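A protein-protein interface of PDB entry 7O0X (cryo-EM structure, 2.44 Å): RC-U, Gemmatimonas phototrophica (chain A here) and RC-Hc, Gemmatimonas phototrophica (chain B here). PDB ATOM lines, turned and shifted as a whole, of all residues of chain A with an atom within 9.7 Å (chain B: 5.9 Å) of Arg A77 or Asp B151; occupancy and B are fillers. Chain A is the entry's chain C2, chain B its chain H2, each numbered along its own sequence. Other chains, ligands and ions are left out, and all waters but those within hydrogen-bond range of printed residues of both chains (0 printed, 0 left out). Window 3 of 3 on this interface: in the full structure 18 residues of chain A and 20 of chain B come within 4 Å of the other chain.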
ATOM      1  N   TRP A  69      12.040  14.550   9.105  1.00  0.00           N
ATOM      2  CA  TRP A  69      13.191  13.783   9.579  1.00  0.00           C
ATOM      3  C   TRP A  69      13.763  12.875   8.495  1.00  0.00           C
ATOM      4  O   TRP A  69      14.982  12.818   8.300  1.00  0.00           O
ATOM      5  CB  TRP A  69      12.810  12.937  10.792  1.00  0.00           C
ATOM      6  CG  TRP A  69      13.914  11.993  11.157  1.00  0.00           C
ATOM      7  CD1 TRP A  69      15.053  12.292  11.844  1.00  0.00           C
ATOM      8  CD2 TRP A  69      14.030  10.618  10.769  1.00  0.00           C
ATOM      9  NE1 TRP A  69      15.849  11.177  11.948  1.00  0.00           N
ATOM     10  CE2 TRP A  69      15.246  10.138  11.290  1.00  0.00           C
ATOM     11  CE3 TRP A  69      13.215   9.743  10.043  1.00  0.00           C
ATOM     12  CZ2 TRP A  69      15.666   8.821  11.112  1.00  0.00           C
ATOM     13  CZ3 TRP A  69      13.634   8.437   9.867  1.00  0.00           C
ATOM     14  CH2 TRP A  69      14.847   7.989  10.399  1.00  0.00           C
ATOM     15  N   ALA A  70      12.899  12.148   7.786  1.00  0.00           N
ATOM     16  CA  ALA A  70      13.364  11.277   6.709  1.00  0.00           C
ATOM     17  C   ALA A  70      14.040  12.053   5.585  1.00  0.00           C
ATOM     18  O   ALA A  70      15.032  11.585   5.012  1.00  0.00           O
ATOM     19  CB  ALA A  70      12.195  10.458   6.162  1.00  0.00           C
ATOM     20  N   LEU A  71      13.526  13.236   5.251  1.00  0.00           N
ATOM     21  CA  LEU A  71      14.217  14.100   4.296  1.00  0.00           C
ATOM     22  C   LEU A  71      15.598  14.509   4.796  1.00  0.00           C
ATOM     23  O   LEU A  71      16.581  14.454   4.048  1.00  0.00           O
ATOM     24  CB  LEU A  71      13.364  15.332   3.993  1.00  0.00           C
ATOM     25  CG  LEU A  71      13.983  16.325   3.008  1.00  0.00           C
ATOM     26  CD1 LEU A  71      14.231  15.665   1.666  1.00  0.00           C
ATOM     27  CD2 LEU A  71      13.081  17.532   2.843  1.00  0.00           C
ATOM     28  N   ALA A  72      15.691  14.935   6.057  1.00  0.00           N
ATOM     29  CA  ALA A  72      16.986  15.301   6.625  1.00  0.00           C
ATOM     30  C   ALA A  72      17.978  14.140   6.600  1.00  0.00           C
ATOM     31  O   ALA A  72      19.159  14.335   6.293  1.00  0.00           O
ATOM     32  CB  ALA A  72      16.800  15.815   8.051  1.00  0.00           C
ATOM     33  N   ASP A  73      17.521  12.926   6.919  1.00  0.00           N
ATOM     34  CA  ASP A  73      18.395  11.756   6.838  1.00  0.00           C
ATOM     35  C   ASP A  73      18.878  11.491   5.416  1.00  0.00           C
ATOM     36  O   ASP A  73      20.064  11.224   5.192  1.00  0.00           O
ATOM     37  CB  ASP A  73      17.675  10.523   7.376  1.00  0.00           C
ATOM     38  CG  ASP A  73      18.532   9.275   7.295  1.00  0.00           C
ATOM     39  OD1 ASP A  73      19.599   9.239   7.941  1.00  0.00           O
ATOM     40  OD2 ASP A  73      18.150   8.338   6.565  1.00  0.00           O
ATOM     41  N   VAL A  74      17.973  11.548   4.440  1.00  0.00           N
ATOM     42  CA  VAL A  74      18.346  11.165   3.083  1.00  0.00           C
ATOM     43  C   VAL A  74      19.113  12.276   2.369  1.00  0.00           C
ATOM     44  O   VAL A  74      19.925  11.999   1.480  1.00  0.00           O
ATOM     45  CB  VAL A  74      17.100  10.721   2.296  1.00  0.00           C
ATOM     46  CG1 VAL A  74      16.380  11.908   1.677  1.00  0.00           C
ATOM     47  CG2 VAL A  74      17.485   9.705   1.241  1.00  0.00           C
ATOM     48  N   GLN A  75      18.877  13.537   2.737  1.00  0.00           N
ATOM     49  CA  GLN A  75      19.767  14.614   2.315  1.00  0.00           C
ATOM     50  C   GLN A  75      21.180  14.422   2.852  1.00  0.00           C
ATOM     51  O   GLN A  75      22.158  14.608   2.119  1.00  0.00           O
ATOM     52  CB  GLN A  75      19.209  15.964   2.767  1.00  0.00           C
ATOM     53  CG  GLN A  75      18.092  16.505   1.894  1.00  0.00           C
ATOM     54  CD  GLN A  75      17.564  17.837   2.386  1.00  0.00           C
ATOM     55  OE1 GLN A  75      17.929  18.302   3.464  1.00  0.00           O
ATOM     56  NE2 GLN A  75      16.702  18.462   1.592  1.00  0.00           N
ATOM     57  N   ALA A  76      21.309  14.061   4.131  1.00  0.00           N
ATOM     58  CA  ALA A  76      22.631  13.848   4.711  1.00  0.00           C
ATOM     59  C   ALA A  76      23.413  12.748   3.998  1.00  0.00           C
ATOM     60  O   ALA A  76      24.611  12.907   3.738  1.00  0.00           O
ATOM     61  CB  ALA A  76      22.497  13.524   6.199  1.00  0.00           C
ATOM     62  N   ARG A  77      22.769  11.627   3.675  1.00  0.00           N
ATOM     63  CA  ARG A  77      23.463  10.590   2.914  1.00  0.00           C
ATOM     64  C   ARG A  77      23.455  10.820   1.400  1.00  0.00           C
ATOM     65  O   ARG A  77      24.093  10.050   0.675  1.00  0.00           O
ATOM     66  CB  ARG A  77      22.935   9.204   3.318  1.00  0.00           C
ATOM     67  CG  ARG A  77      21.614   8.730   2.767  1.00  0.00           C
ATOM     68  CD  ARG A  77      21.292   7.368   3.397  1.00  0.00           C
ATOM     69  NE  ARG A  77      20.834   7.490   4.779  1.00  0.00           N
ATOM     70  CZ  ARG A  77      21.072   6.602   5.736  1.00  0.00           C
ATOM     71  NH1 ARG A  77      21.765   5.500   5.502  1.00  0.00           N
ATOM     72  NH2 ARG A  77      20.606   6.826   6.961  1.00  0.00           N
ATOM     73  N   GLY A  78      22.765  11.852   0.908  1.00  0.00           N
ATOM     74  CA  GLY A  78      23.041  12.422  -0.404  1.00  0.00           C
ATOM     75  C   GLY A  78      22.468  11.752  -1.637  1.00  0.00           C
ATOM     76  O   GLY A  78      22.796  12.183  -2.748  1.00  0.00           O
ATOM     77  N   ILE A  79      21.635  10.724  -1.505  1.00  0.00           N
ATOM     78  CA  ILE A  79      21.168   9.967  -2.667  1.00  0.00           C
ATOM     79  C   ILE A  79      20.085  10.768  -3.392  1.00  0.00           C
ATOM     80  O   ILE A  79      18.965  10.905  -2.896  1.00  0.00           O
ATOM     81  CB  ILE A  79      20.657   8.579  -2.271  1.00  0.00           C
ATOM     82  CG1 ILE A  79      21.731   7.826  -1.485  1.00  0.00           C
ATOM     83  CG2 ILE A  79      20.268   7.791  -3.510  1.00  0.00           C
ATOM     84  CD1 ILE A  79      21.271   6.486  -0.961  1.00  0.00           C
ATOM     85  N   VAL A  80      20.422  11.292  -4.570  1.00  0.00           N
ATOM     86  CA  VAL A  80      19.611  12.264  -5.312  1.00  0.00           C
ATOM     87  C   VAL A  80      18.177  11.802  -5.583  1.00  0.00           C
ATOM     88  O   VAL A  80      17.240  12.521  -5.205  1.00  0.00           O
ATOM     89  CB  VAL A  80      20.309  12.662  -6.624  1.00  0.00           C
ATOM     90  CG1 VAL A  80      19.366  13.456  -7.514  1.00  0.00           C
ATOM     91  CG2 VAL A  80      21.563  13.465  -6.330  1.00  0.00           C
ATOM     92  N   PRO A  81      17.930  10.650  -6.226  1.00  0.00           N
ATOM     93  CA  PRO A  81      16.532  10.270  -6.504  1.00  0.00           C
ATOM     94  C   PRO A  81      15.707  10.002  -5.258  1.00  0.00           C
ATOM     95  O   PRO A  81      14.476  10.108  -5.314  1.00  0.00           O
ATOM     96  CB  PRO A  81      16.670   9.002  -7.361  1.00  0.00           C
ATOM     97  CG  PRO A  81      17.985   8.446  -6.987  1.00  0.00           C
ATOM     98  CD  PRO A  81      18.865   9.636  -6.747  1.00  0.00           C
ATOM     99  N   CYS A  82      16.344   9.657  -4.141  1.00  0.00           N
ATOM    100  CA  CYS A  82      15.635   9.493  -2.877  1.00  0.00           C
ATOM    101  C   CYS A  82      15.301  10.834  -2.231  1.00  0.00           C
ATOM    102  O   CYS A  82      14.224  10.993  -1.650  1.00  0.00           O
ATOM    103  CB  CYS A  82      16.459   8.621  -1.932  1.00  0.00           C
ATOM    104  SG  CYS A  82      16.883   7.007  -2.622  1.00  0.00           S
ATOM    105  N   ILE A  83      16.215  11.805  -2.318  1.00  0.00           N
ATOM    106  CA  ILE A  83      15.929  13.159  -1.846  1.00  0.00           C
ATOM    107  C   ILE A  83      14.715  13.741  -2.564  1.00  0.00           C
ATOM    108  O   ILE A  83      13.860  14.385  -1.943  1.00  0.00           O
ATOM    109  CB  ILE A  83      17.167  14.058  -2.023  1.00  0.00           C
ATOM    110  CG1 ILE A  83      18.300  13.611  -1.100  1.00  0.00           C
ATOM    111  CG2 ILE A  83      16.817  15.515  -1.761  1.00  0.00           C
ATOM    112  CD1 ILE A  83      19.659  14.127  -1.520  1.00  0.00           C
ATOM    113  N   HIS B  49      20.334  -5.446  -1.491  1.00  0.00           N
ATOM    114  CA  HIS B  49      19.759  -5.783  -0.191  1.00  0.00           C
ATOM    115  C   HIS B  49      18.250  -5.966  -0.300  1.00  0.00           C
ATOM    116  O   HIS B  49      17.546  -5.116  -0.849  1.00  0.00           O
ATOM    117  CB  HIS B  49      20.083  -4.703   0.840  1.00  0.00           C
ATOM    118  CG  HIS B  49      21.548  -4.502   1.071  1.00  0.00           C
ATOM    119  ND1 HIS B  49      22.083  -3.292   1.455  1.00  0.00           N
ATOM    120  CD2 HIS B  49      22.587  -5.365   0.992  1.00  0.00           C
ATOM    121  CE1 HIS B  49      23.391  -3.417   1.593  1.00  0.00           C
ATOM    122  NE2 HIS B  49      23.722  -4.665   1.318  1.00  0.00           N
ATOM    123  N   ILE B  51      15.869  -6.285   2.255  1.00  0.00           N
ATOM    124  CA  ILE B  51      15.022  -5.570   3.203  1.00  0.00           C
ATOM    125  C   ILE B  51      15.695  -4.258   3.568  1.00  0.00           C
ATOM    126  O   ILE B  51      16.795  -4.249   4.134  1.00  0.00           O
ATOM    127  CB  ILE B  51      14.732  -6.413   4.454  1.00  0.00           C
ATOM    128  CG1 ILE B  51      14.146  -7.765   4.046  1.00  0.00           C
ATOM    129  CG2 ILE B  51      13.786  -5.676   5.386  1.00  0.00           C
ATOM    130  CD1 ILE B  51      13.736  -8.631   5.206  1.00  0.00           C
ATOM    131  N   VAL B  52      15.023  -3.155   3.251  1.00  0.00           N
ATOM    132  CA  VAL B  52      15.591  -1.811   3.372  1.00  0.00           C
ATOM    133  C   VAL B  52      14.513  -0.860   3.849  1.00  0.00           C
ATOM    134  O   VAL B  52      13.315  -1.083   3.630  1.00  0.00           O
ATOM    135  CB  VAL B  52      16.165  -1.307   2.029  1.00  0.00           C
ATOM    136  CG1 VAL B  52      17.351  -2.150   1.594  1.00  0.00           C
ATOM    137  CG2 VAL B  52      15.087  -1.305   0.959  1.00  0.00           C
ATOM    138  N   PRO B  53      14.911   0.216   4.523  1.00  0.00           N
ATOM    139  CA  PRO B  53      13.951   1.289   4.804  1.00  0.00           C
ATOM    140  C   PRO B  53      13.419   1.900   3.515  1.00  0.00           C
ATOM    141  O   PRO B  53      14.166   2.150   2.568  1.00  0.00           O
ATOM    142  CB  PRO B  53      14.765   2.294   5.626  1.00  0.00           C
ATOM    143  CG  PRO B  53      16.179   2.021   5.282  1.00  0.00           C
ATOM    144  CD  PRO B  53      16.265   0.549   4.999  1.00  0.00           C
ATOM    145  N   ARG B  55      12.400   4.741   2.731  1.00  0.00           N
ATOM    146  CA  ARG B  55      13.128   5.971   2.436  1.00  0.00           C
ATOM    147  C   ARG B  55      14.242   5.800   1.407  1.00  0.00           C
ATOM    148  O   ARG B  55      14.558   6.747   0.678  1.00  0.00           O
ATOM    149  CB  ARG B  55      13.707   6.474   3.757  1.00  0.00           C
ATOM    150  CG  ARG B  55      14.541   7.714   3.760  1.00  0.00           C
ATOM    151  CD  ARG B  55      14.824   8.049   5.219  1.00  0.00           C
ATOM    152  NE  ARG B  55      15.954   7.292   5.744  1.00  0.00           N
ATOM    153  CZ  ARG B  55      15.877   6.357   6.682  1.00  0.00           C
ATOM    154  NH1 ARG B  55      14.744   5.727   6.940  1.00  0.00           N
ATOM    155  NH2 ARG B  55      16.989   5.964   7.296  1.00  0.00           N
ATOM    156  N   LEU B  56      14.842   4.615   1.318  1.00  0.00           N
ATOM    157  CA  LEU B  56      15.956   4.375   0.409  1.00  0.00           C
ATOM    158  C   LEU B  56      15.588   3.582  -0.842  1.00  0.00           C
ATOM    159  O   LEU B  56      16.490   3.166  -1.575  1.00  0.00           O
ATOM    160  CB  LEU B  56      17.093   3.678   1.153  1.00  0.00           C
ATOM    161  CG  LEU B  56      17.529   4.367   2.445  1.00  0.00           C
ATOM    162  CD1 LEU B  56      18.703   3.638   3.044  1.00  0.00           C
ATOM    163  CD2 LEU B  56      17.880   5.824   2.193  1.00  0.00           C
ATOM    164  N   TRP B  89      10.130  -0.545   6.727  1.00  0.00           N
ATOM    165  CA  TRP B  89      11.113  -1.336   5.997  1.00  0.00           C
ATOM    166  C   TRP B  89      10.382  -2.312   5.083  1.00  0.00           C
ATOM    167  O   TRP B  89       9.469  -3.015   5.527  1.00  0.00           O
ATOM    168  CB  TRP B  89      12.029  -2.100   6.955  1.00  0.00           C
ATOM    169  CG  TRP B  89      12.979  -1.243   7.744  1.00  0.00           C
ATOM    170  CD1 TRP B  89      12.663  -0.167   8.520  1.00  0.00           C
ATOM    171  CD2 TRP B  89      14.395  -1.420   7.863  1.00  0.00           C
ATOM    172  NE1 TRP B  89      13.796   0.347   9.100  1.00  0.00           N
ATOM    173  CE2 TRP B  89      14.874  -0.406   8.713  1.00  0.00           C
ATOM    174  CE3 TRP B  89      15.307  -2.334   7.326  1.00  0.00           C
ATOM    175  CZ2 TRP B  89      16.222  -0.279   9.040  1.00  0.00           C
ATOM    176  CZ3 TRP B  89      16.644  -2.207   7.652  1.00  0.00           C
ATOM    177  CH2 TRP B  89      17.088  -1.189   8.500  1.00  0.00           C
ATOM    178  N   ARG B 149      23.447  -1.296  11.467  1.00  0.00           N
ATOM    179  CA  ARG B 149      23.354  -0.155  10.559  1.00  0.00           C
ATOM    180  C   ARG B 149      21.889   0.228  10.415  1.00  0.00           C
ATOM    181  O   ARG B 149      20.993  -0.583  10.655  1.00  0.00           O
ATOM    182  CB  ARG B 149      23.949  -0.431   9.168  1.00  0.00           C
ATOM    183  CG  ARG B 149      25.396  -0.880   9.143  1.00  0.00           C
ATOM    184  CD  ARG B 149      25.985  -0.720   7.745  1.00  0.00           C
ATOM    185  NE  ARG B 149      26.548   0.609   7.538  1.00  0.00           N
ATOM    186  CZ  ARG B 149      26.255   1.409   6.520  1.00  0.00           C
ATOM    187  NH1 ARG B 149      25.253   1.144   5.698  1.00  0.00           N
ATOM    188  NH2 ARG B 149      26.946   2.533   6.359  1.00  0.00           N
ATOM    189  N   ASP B 150      21.640   1.473  10.013  1.00  0.00           N
ATOM    190  CA  ASP B 150      20.274   1.971   9.921  1.00  0.00           C
ATOM    191  C   ASP B 150      19.652   1.790   8.538  1.00  0.00           C
ATOM    192  O   ASP B 150      18.549   2.293   8.299  1.00  0.00           O
ATOM    193  CB  ASP B 150      20.208   3.441  10.366  1.00  0.00           C
ATOM    194  CG  ASP B 150      20.828   4.408   9.364  1.00  0.00           C
ATOM    195  OD1 ASP B 150      21.418   3.975   8.353  1.00  0.00           O
ATOM    196  OD2 ASP B 150      20.717   5.631   9.600  1.00  0.00           O
ATOM    197  N   ASP B 151      20.328   1.092   7.626  1.00  0.00           N
ATOM    198  CA  ASP B 151      19.861   0.971   6.254  1.00  0.00           C
ATOM    199  C   ASP B 151      19.883  -0.459   5.729  1.00  0.00           C
ATOM    200  O   ASP B 151      19.583  -0.673   4.550  1.00  0.00           O
ATOM    201  CB  ASP B 151      20.682   1.879   5.323  1.00  0.00           C
ATOM    202  CG  ASP B 151      22.156   1.529   5.297  1.00  0.00           C
ATOM    203  OD1 ASP B 151      22.580   0.612   6.030  1.00  0.00           O
ATOM    204  OD2 ASP B 151      22.898   2.184   4.536  1.00  0.00           O
ATOM    205  N   GLN B 152      20.232  -1.435   6.563  1.00  0.00           N
ATOM    206  CA  GLN B 152      20.219  -2.840   6.181  1.00  0.00           C
ATOM    207  C   GLN B 152      20.082  -3.677   7.444  1.00  0.00           C
ATOM    208  O   GLN B 152      20.374  -3.212   8.548  1.00  0.00           O
ATOM    209  CB  GLN B 152      21.489  -3.211   5.411  1.00  0.00           C
ATOM    210  CG  GLN B 152      22.760  -3.017   6.221  1.00  0.00           C
ATOM    211  CD  GLN B 152      24.013  -3.303   5.422  1.00  0.00           C
ATOM    212  OE1 GLN B 152      24.333  -2.594   4.470  1.00  0.00           O
ATOM    213  NE2 GLN B 152      24.737  -4.343   5.813  1.00  0.00           N
ATOM    214  N   ILE B 153      19.630  -4.917   7.272  1.00  0.00           N
ATOM    215  CA  ILE B 153      19.478  -5.846   8.387  1.00  0.00           C
ATOM    216  C   ILE B 153      19.985  -7.219   7.963  1.00  0.00           C
ATOM    217  O   ILE B 153      19.678  -7.689   6.863  1.00  0.00           O
ATOM    218  CB  ILE B 153      18.016  -5.908   8.881  1.00  0.00           C
ATOM    219  CG1 ILE B 153      17.882  -6.854  10.074  1.00  0.00           C
ATOM    220  CG2 ILE B 153      17.063  -6.285   7.752  1.00  0.00           C
ATOM    221  CD1 ILE B 153      16.569  -6.715  10.813  1.00  0.00           C
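Printed residues of chain B within 4 Å of Ala A70: Arg B55 (3.5 Å).
Ala A72 touches none of the printed residues of chain B.
Printed residues of chain B within 4 Å of Asp A73: Arg B55 (2.6 Å).
Arg A77 touches four residues of chain B.
Printed residues of chain B within 4 Å of Cys A82: Arg B55 (3.7 Å).
Ile A83 touches none of the printed residues of chain B.
Of the printed residues of chain A, Leu B56 touches Arg A77 (3.9 Å).
Asp B150 touches just one residue of chain A: Arg A77 (2.9 Å).
No residue of chain A comes within 4 Å of Gln B152.
The nearest residue of chain B that does not touch Arg A77 is Arg B149 (5.6 Å).
The nearest residue of chain A that does not touch Asp B151 is Asp A73 (7.0 Å).
The nearest printed residue of chain B that does not touch Ala A70 is Leu B56 (7.0 Å).
Of the 15 printed residues of chain A, 4 touch a printed residue of chain B.
Printed residues of chain A that touch a printed residue of chain B: Ala A70, Asp A73, Arg A77 and Cys A82.
Hydrophobic or aromatic side chains of chain A within 4 Å of the printed part of chain B: Ala A70.
Among the printed residues, 7 pairs touch across the chains.
The guanidinium group (NH2) of Arg A77 is in salt-bridge range of the side-chain carboxylate (OD1) of Asp A73 (2.8 Å).
The guanidinium group of Arg B149 lies within salt-bridge range of the side-chain carboxylate of Asp B151 (2.7 Å).
Ala A70 touches Arg B55 (O to CD, 3.5 Å).
Arg A77 touches Arg B55 (NH2 to NH2, 3.7 Å).
Arg A77 touches Leu B56.
CB of Cys A82 touches O of Arg B55, at 3.7 Å.
OD2 of Asp A73 is in salt-bridge range of NE of Arg B55, at 2.6 Å.
NH1 of Arg A77 lies within salt-bridge range of OD2 of Asp B151 (3.6 Å).
The guanidinium group of Arg A77 lies within salt-bridge range of the side-chain carboxylate of Asp B150, 2.9 Å away.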
